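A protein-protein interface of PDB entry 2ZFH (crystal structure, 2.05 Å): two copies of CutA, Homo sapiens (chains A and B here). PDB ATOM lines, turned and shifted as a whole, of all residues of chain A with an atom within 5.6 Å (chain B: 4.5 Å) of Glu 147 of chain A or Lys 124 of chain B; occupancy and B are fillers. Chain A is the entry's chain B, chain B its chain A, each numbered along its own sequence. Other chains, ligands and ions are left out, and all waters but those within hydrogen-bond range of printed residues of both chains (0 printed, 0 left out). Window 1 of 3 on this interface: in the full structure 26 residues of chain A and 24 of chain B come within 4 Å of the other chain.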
ATOM      1  N   PHE A  72       6.046  28.544 -16.158  1.00  0.00           N
ATOM      2  CA  PHE A  72       6.417  27.224 -16.639  1.00  0.00           C
ATOM      3  C   PHE A  72       5.178  26.378 -16.917  1.00  0.00           C
ATOM      4  O   PHE A  72       4.276  26.274 -16.081  1.00  0.00           O
ATOM      5  CB  PHE A  72       7.310  26.500 -15.631  1.00  0.00           C
ATOM      6  CG  PHE A  72       8.695  27.063 -15.541  1.00  0.00           C
ATOM      7  CD1 PHE A  72       8.963  28.168 -14.740  1.00  0.00           C
ATOM      8  CD2 PHE A  72       9.729  26.515 -16.290  1.00  0.00           C
ATOM      9  CE1 PHE A  72      10.241  28.712 -14.688  1.00  0.00           C
ATOM     10  CE2 PHE A  72      11.008  27.054 -16.241  1.00  0.00           C
ATOM     11  CZ  PHE A  72      11.261  28.155 -15.438  1.00  0.00           C
ATOM     12  N   VAL A  73       5.149  25.787 -18.109  1.00  0.00           N
ATOM     13  CA  VAL A  73       4.058  24.928 -18.551  1.00  0.00           C
ATOM     14  C   VAL A  73       4.628  23.606 -19.082  1.00  0.00           C
ATOM     15  O   VAL A  73       5.661  23.575 -19.752  1.00  0.00           O
ATOM     16  CB  VAL A  73       3.249  25.594 -19.684  1.00  0.00           C
ATOM     17  CG1 VAL A  73       2.111  24.685 -20.121  1.00  0.00           C
ATOM     18  CG2 VAL A  73       2.712  26.927 -19.219  1.00  0.00           C
ATOM     19  N   THR A  74       3.955  22.513 -18.779  1.00  0.00           N
ATOM     20  CA  THR A  74       4.408  21.217 -19.252  1.00  0.00           C
ATOM     21  C   THR A  74       3.437  20.697 -20.293  1.00  0.00           C
ATOM     22  O   THR A  74       2.233  20.716 -20.086  1.00  0.00           O
ATOM     23  CB  THR A  74       4.487  20.203 -18.108  1.00  0.00           C
ATOM     24  OG1 THR A  74       5.348  20.709 -17.084  1.00  0.00           O
ATOM     25  CG2 THR A  74       5.043  18.898 -18.606  1.00  0.00           C
ATOM     26  N   LEU A 120       8.904  21.070 -21.694  1.00  0.00           N
ATOM     27  CA  LEU A 120       8.703  22.132 -20.719  1.00  0.00           C
ATOM     28  C   LEU A 120       8.762  23.486 -21.421  1.00  0.00           C
ATOM     29  O   LEU A 120       9.636  23.734 -22.239  1.00  0.00           O
ATOM     30  CB  LEU A 120       9.782  22.045 -19.633  1.00  0.00           C
ATOM     31  CG  LEU A 120       9.739  23.035 -18.466  1.00  0.00           C
ATOM     32  CD1 LEU A 120       8.473  22.805 -17.630  1.00  0.00           C
ATOM     33  CD2 LEU A 120      10.993  22.851 -17.615  1.00  0.00           C
ATOM     34  N   HIS A 141      -5.237  23.083 -23.662  1.00  0.00           N
ATOM     35  CA  HIS A 141      -4.288  22.059 -23.246  1.00  0.00           C
ATOM     36  C   HIS A 141      -5.000  20.720 -23.169  1.00  0.00           C
ATOM     37  O   HIS A 141      -6.111  20.624 -22.646  1.00  0.00           O
ATOM     38  CB  HIS A 141      -3.676  22.418 -21.887  1.00  0.00           C
ATOM     39  CG  HIS A 141      -2.329  21.807 -21.647  1.00  0.00           C
ATOM     40  ND1 HIS A 141      -2.163  20.518 -21.187  1.00  0.00           N
ATOM     41  CD2 HIS A 141      -1.082  22.308 -21.820  1.00  0.00           C
ATOM     42  CE1 HIS A 141      -0.872  20.253 -21.087  1.00  0.00           C
ATOM     43  NE2 HIS A 141      -0.195  21.322 -21.466  1.00  0.00           N
ATOM     44  N   TYR A 143      -4.299  18.046 -21.348  1.00  0.00           N
ATOM     45  CA  TYR A 143      -4.438  17.495 -19.998  1.00  0.00           C
ATOM     46  C   TYR A 143      -5.662  18.053 -19.272  1.00  0.00           C
ATOM     47  O   TYR A 143      -6.132  19.153 -19.568  1.00  0.00           O
ATOM     48  CB  TYR A 143      -3.202  17.796 -19.134  1.00  0.00           C
ATOM     49  CG  TYR A 143      -1.874  17.283 -19.654  1.00  0.00           C
ATOM     50  CD1 TYR A 143      -1.808  16.222 -20.558  1.00  0.00           C
ATOM     51  CD2 TYR A 143      -0.676  17.848 -19.209  1.00  0.00           C
ATOM     52  CE1 TYR A 143      -0.576  15.737 -21.009  1.00  0.00           C
ATOM     53  CE2 TYR A 143       0.560  17.373 -19.652  1.00  0.00           C
ATOM     54  CZ  TYR A 143       0.603  16.318 -20.551  1.00  0.00           C
ATOM     55  OH  TYR A 143       1.818  15.852 -20.992  1.00  0.00           O
ATOM     56  N   VAL A 145      -5.726  18.724 -15.984  1.00  0.00           N
ATOM     57  CA  VAL A 145      -5.194  19.778 -15.125  1.00  0.00           C
ATOM     58  C   VAL A 145      -3.787  20.152 -15.591  1.00  0.00           C
ATOM     59  O   VAL A 145      -2.803  19.501 -15.234  1.00  0.00           O
ATOM     60  CB  VAL A 145      -5.129  19.332 -13.652  1.00  0.00           C
ATOM     61  CG1 VAL A 145      -4.573  20.454 -12.798  1.00  0.00           C
ATOM     62  CG2 VAL A 145      -6.520  18.935 -13.169  1.00  0.00           C
ATOM     63  N   ALA A 146      -3.704  21.206 -16.392  1.00  0.00           N
ATOM     64  CA  ALA A 146      -2.428  21.664 -16.924  1.00  0.00           C
ATOM     65  C   ALA A 146      -1.522  22.319 -15.879  1.00  0.00           C
ATOM     66  O   ALA A 146      -1.963  23.126 -15.060  1.00  0.00           O
ATOM     67  CB  ALA A 146      -2.670  22.630 -18.077  1.00  0.00           C
ATOM     68  N   GLU A 147      -0.249  21.958 -15.913  1.00  0.00           N
ATOM     69  CA  GLU A 147       0.710  22.539 -14.996  1.00  0.00           C
ATOM     70  C   GLU A 147       1.021  23.951 -15.439  1.00  0.00           C
ATOM     71  O   GLU A 147       1.534  24.164 -16.535  1.00  0.00           O
ATOM     72  CB  GLU A 147       2.019  21.761 -14.994  1.00  0.00           C
ATOM     73  CG  GLU A 147       3.107  22.462 -14.187  1.00  0.00           C
ATOM     74  CD  GLU A 147       4.504  21.946 -14.482  1.00  0.00           C
ATOM     75  OE1 GLU A 147       4.721  20.714 -14.396  1.00  0.00           O
ATOM     76  OE2 GLU A 147       5.386  22.783 -14.794  1.00  0.00           O
ATOM     77  N   VAL A 148       0.697  24.919 -14.602  1.00  0.00           N
ATOM     78  CA  VAL A 148       1.023  26.297 -14.915  1.00  0.00           C
ATOM     79  C   VAL A 148       1.483  26.971 -13.633  1.00  0.00           C
ATOM     80  O   VAL A 148       0.712  27.125 -12.697  1.00  0.00           O
ATOM     81  CB  VAL A 148      -0.175  27.058 -15.497  1.00  0.00           C
ATOM     82  CG1 VAL A 148       0.226  28.495 -15.799  1.00  0.00           C
ATOM     83  CG2 VAL A 148      -0.645  26.375 -16.767  1.00  0.00           C
ATOM     84  N   ILE A 149       2.761  27.328 -13.578  1.00  0.00           N
ATOM     85  CA  ILE A 149       3.302  28.002 -12.406  1.00  0.00           C
ATOM     86  C   ILE A 149       4.092  29.205 -12.884  1.00  0.00           C
ATOM     87  O   ILE A 149       4.786  29.142 -13.900  1.00  0.00           O
ATOM     88  CB  ILE A 149       4.222  27.078 -11.566  1.00  0.00           C
ATOM     89  CG1 ILE A 149       5.446  26.662 -12.378  1.00  0.00           C
ATOM     90  CG2 ILE A 149       3.453  25.841 -11.119  1.00  0.00           C
ATOM     91  CD1 ILE A 149       6.445  25.870 -11.569  1.00  0.00           C
ATOM     92  N   SER B  69       6.522  26.053  -4.038  1.00  0.00           N
ATOM     93  CA  SER B  69       7.809  26.457  -4.590  1.00  0.00           C
ATOM     94  C   SER B  69       8.335  25.492  -5.644  1.00  0.00           C
ATOM     95  O   SER B  69       7.880  24.355  -5.753  1.00  0.00           O
ATOM     96  CB  SER B  69       8.858  26.583  -3.479  1.00  0.00           C
ATOM     97  OG  SER B  69       8.579  27.683  -2.634  1.00  0.00           O
ATOM     98  N   ALA B  94       7.594  15.843  -2.431  1.00  0.00           N
ATOM     99  CA  ALA B  94       7.375  16.557  -3.683  1.00  0.00           C
ATOM    100  C   ALA B  94       6.227  15.919  -4.441  1.00  0.00           C
ATOM    101  O   ALA B  94       5.969  14.716  -4.318  1.00  0.00           O
ATOM    102  CB  ALA B  94       8.626  16.519  -4.537  1.00  0.00           C
ATOM    103  N   ALA B  95       5.547  16.726  -5.243  1.00  0.00           N
ATOM    104  CA  ALA B  95       4.424  16.242  -6.022  1.00  0.00           C
ATOM    105  C   ALA B  95       4.831  15.955  -7.450  1.00  0.00           C
ATOM    106  O   ALA B  95       4.208  15.138  -8.125  1.00  0.00           O
ATOM    107  CB  ALA B  95       3.317  17.268  -6.010  1.00  0.00           C
ATOM    108  N   CYS B  96       5.885  16.620  -7.910  1.00  0.00           N
ATOM    109  CA  CYS B  96       6.318  16.454  -9.285  1.00  0.00           C
ATOM    110  C   CYS B  96       7.776  16.842  -9.509  1.00  0.00           C
ATOM    111  O   CYS B  96       8.264  17.818  -8.942  1.00  0.00           O
ATOM    112  CB  CYS B  96       5.414  17.307 -10.184  1.00  0.00           C
ATOM    113  SG  CYS B  96       5.789  17.215 -11.939  1.00  0.00           S
ATOM    114  N   ASN B  98      10.627  17.307 -12.758  1.00  0.00           N
ATOM    115  CA  ASN B  98      10.891  17.367 -14.196  1.00  0.00           C
ATOM    116  C   ASN B  98      12.395  17.218 -14.360  1.00  0.00           C
ATOM    117  O   ASN B  98      13.162  17.972 -13.761  1.00  0.00           O
ATOM    118  CB  ASN B  98      10.461  18.717 -14.770  1.00  0.00           C
ATOM    119  CG  ASN B  98       8.962  18.863 -14.857  1.00  0.00           C
ATOM    120  OD1 ASN B  98       8.448  19.969 -14.968  1.00  0.00           O
ATOM    121  ND2 ASN B  98       8.251  17.747 -14.825  1.00  0.00           N
ATOM    122  N   MET B 122      13.784  19.925 -11.636  1.00  0.00           N
ATOM    123  CA  MET B 122      12.896  21.006 -11.241  1.00  0.00           C
ATOM    124  C   MET B 122      11.860  20.295 -10.374  1.00  0.00           C
ATOM    125  O   MET B 122      11.146  19.409 -10.840  1.00  0.00           O
ATOM    126  CB  MET B 122      12.244  21.672 -12.458  1.00  0.00           C
ATOM    127  CG  MET B 122      11.297  22.810 -12.073  1.00  0.00           C
ATOM    128  SD  MET B 122      10.895  23.924 -13.431  1.00  0.00           S
ATOM    129  CE  MET B 122      10.386  25.370 -12.533  1.00  0.00           C
ATOM    130  N   ILE B 123      11.797  20.672  -9.103  1.00  0.00           N
ATOM    131  CA  ILE B 123      10.896  20.019  -8.159  1.00  0.00           C
ATOM    132  C   ILE B 123       9.792  20.919  -7.624  1.00  0.00           C
ATOM    133  O   ILE B 123      10.063  21.959  -7.036  1.00  0.00           O
ATOM    134  CB  ILE B 123      11.704  19.457  -6.970  1.00  0.00           C
ATOM    135  CG1 ILE B 123      12.869  18.607  -7.493  1.00  0.00           C
ATOM    136  CG2 ILE B 123      10.817  18.616  -6.097  1.00  0.00           C
ATOM    137  CD1 ILE B 123      13.781  18.025  -6.403  1.00  0.00           C
ATOM    138  N   LYS B 124       8.543  20.510  -7.831  1.00  0.00           N
ATOM    139  CA  LYS B 124       7.401  21.280  -7.365  1.00  0.00           C
ATOM    140  C   LYS B 124       6.870  20.697  -6.072  1.00  0.00           C
ATOM    141  O   LYS B 124       6.438  19.546  -6.023  1.00  0.00           O
ATOM    142  CB  LYS B 124       6.276  21.289  -8.407  1.00  0.00           C
ATOM    143  CG  LYS B 124       6.487  22.230  -9.589  1.00  0.00           C
ATOM    144  CD  LYS B 124       7.623  21.795 -10.496  1.00  0.00           C
ATOM    145  CE  LYS B 124       7.345  20.456 -11.174  1.00  0.00           C
ATOM    146  NZ  LYS B 124       6.099  20.497 -11.989  1.00  0.00           N
ATOM    147  N   THR B 125       6.898  21.498  -5.019  1.00  0.00           N
ATOM    148  CA  THR B 125       6.414  21.041  -3.740  1.00  0.00           C
ATOM    149  C   THR B 125       5.918  22.199  -2.895  1.00  0.00           C
ATOM    150  O   THR B 125       5.947  23.352  -3.322  1.00  0.00           O
ATOM    151  CB  THR B 125       7.510  20.274  -2.966  1.00  0.00           C
ATOM    152  OG1 THR B 125       6.922  19.657  -1.820  1.00  0.00           O
ATOM    153  CG2 THR B 125       8.619  21.207  -2.512  1.00  0.00           C
ATOM    154  N   TYR B 160      -4.031  22.937 -10.264  1.00  0.00           N
ATOM    155  CA  TYR B 160      -2.732  22.275 -10.281  1.00  0.00           C
ATOM    156  C   TYR B 160      -2.022  22.522  -8.952  1.00  0.00           C
ATOM    157  O   TYR B 160      -1.535  21.584  -8.307  1.00  0.00           O
ATOM    158  CB  TYR B 160      -1.868  22.818 -11.419  1.00  0.00           C
ATOM    159  CG  TYR B 160      -0.468  22.237 -11.441  1.00  0.00           C
ATOM    160  CD1 TYR B 160      -0.238  20.933 -11.885  1.00  0.00           C
ATOM    161  CD2 TYR B 160       0.622  22.986 -11.005  1.00  0.00           C
ATOM    162  CE1 TYR B 160       1.042  20.391 -11.898  1.00  0.00           C
ATOM    163  CE2 TYR B 160       1.907  22.455 -11.009  1.00  0.00           C
ATOM    164  CZ  TYR B 160       2.111  21.158 -11.461  1.00  0.00           C
ATOM    165  OH  TYR B 160       3.387  20.645 -11.500  1.00  0.00           O
ATOM    166  N   VAL B 164      -0.750  19.971  -5.956  1.00  0.00           N
ATOM    167  CA  VAL B 164       0.596  19.883  -5.390  1.00  0.00           C
ATOM    168  C   VAL B 164       0.535  19.840  -3.860  1.00  0.00           C
ATOM    169  O   VAL B 164       1.280  19.099  -3.220  1.00  0.00           O
ATOM    170  CB  VAL B 164       1.483  21.093  -5.800  1.00  0.00           C
ATOM    171  CG1 VAL B 164       2.811  21.047  -5.036  1.00  0.00           C
ATOM    172  CG2 VAL B 164       1.727  21.081  -7.297  1.00  0.00           C
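The side-chain carboxylate (OE1) of Glu 147 of chain A is in salt-bridge range of the side-chain amino group (NZ) of Lys 124 of chain B (2.8 Å).
The side-chain hydroxyl (OH) of Tyr 160 of chain B sits at hydrogen-bond distance from the side-chain carboxylate (OE1) of Glu 147 of chain A, at 3.2 Å.
The backbone NH (N) of Ala 95 of chain B lies within hydrogen-bond range of the backbone carbonyl oxygen (O) of Lys 124 of chain B.
O of Cys 96 of chain B lies within hydrogen-bond range of N of Lys 124 of chain B (2.9 Å).
N of Asn 98 of chain B is in hydrogen-bond range of O of Met 122 of chain B (2.9 Å).
OH of Tyr 160 of chain B lies within hydrogen-bond range of NZ of Lys 124 of chain B (2.8 Å).
N of Phe 72 of chain A sits at hydrogen-bond distance from O of Ile 149 of chain A (2.7 Å).
O of Thr 74 of chain A sits at hydrogen-bond distance from NE2 of His 141 of chain A, 2.9 Å away.
Among the printed residues, merely in contact across the chains: Val 145 of chain A with Tyr 160 of chain B (3.6 Å), Ala 146 of chain A with Tyr 160 of chain B (3.7 Å), Ile 149 of chain A with Tyr 160 of chain B (3.7 Å), Thr 74 of chain A with Asn 98 of chain B (3.8 Å), Phe 72 of chain A with Met 122 of chain B (3.8 Å), Glu 147 of chain A with Asn 98 of chain B (3.8 Å) and Leu 120 of chain A with Asn 98 of chain B (3.9 Å).
Glu 147 of chain A touches three residues of chain B.
Lys 124 of chain B touches just one residue of chain A: Glu 147.
Of the printed residues of chain B, Leu 120 of chain A touches Asn 98.
Of the printed residues of chain A, Asn 98 of chain B touches Thr 74, Leu 120 and Glu 147.
Of the printed residues of chain B, Ile 149 of chain A touches Tyr 160.
Printed residues of chain B within 4 Å of Thr 74 of chain A: Asn 98 (3.8 Å).
Ser 69 of chain B touches none of the printed residues of chain A.
Cys 96 of chain B touches none of the printed residues of chain A.
The nearest printed residue of chain A that does not touch Tyr 160 of chain B is Val 148 of chain A (4.1 Å).
Of the 11 printed residues of chain B, 4 touch a printed residue of chain A.
Hydrophobic or aromatic side chains of chain A that line the printed part of chain B: Phe 72, Leu 120, Val 145 and Ile 149.
Among the printed residues, 9 pairs touch across the chains.
No position is printed for both chains.
Of the 9 pairs that touch across the chains among the printed residues, none has its exchanged pair printed and touching as well.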
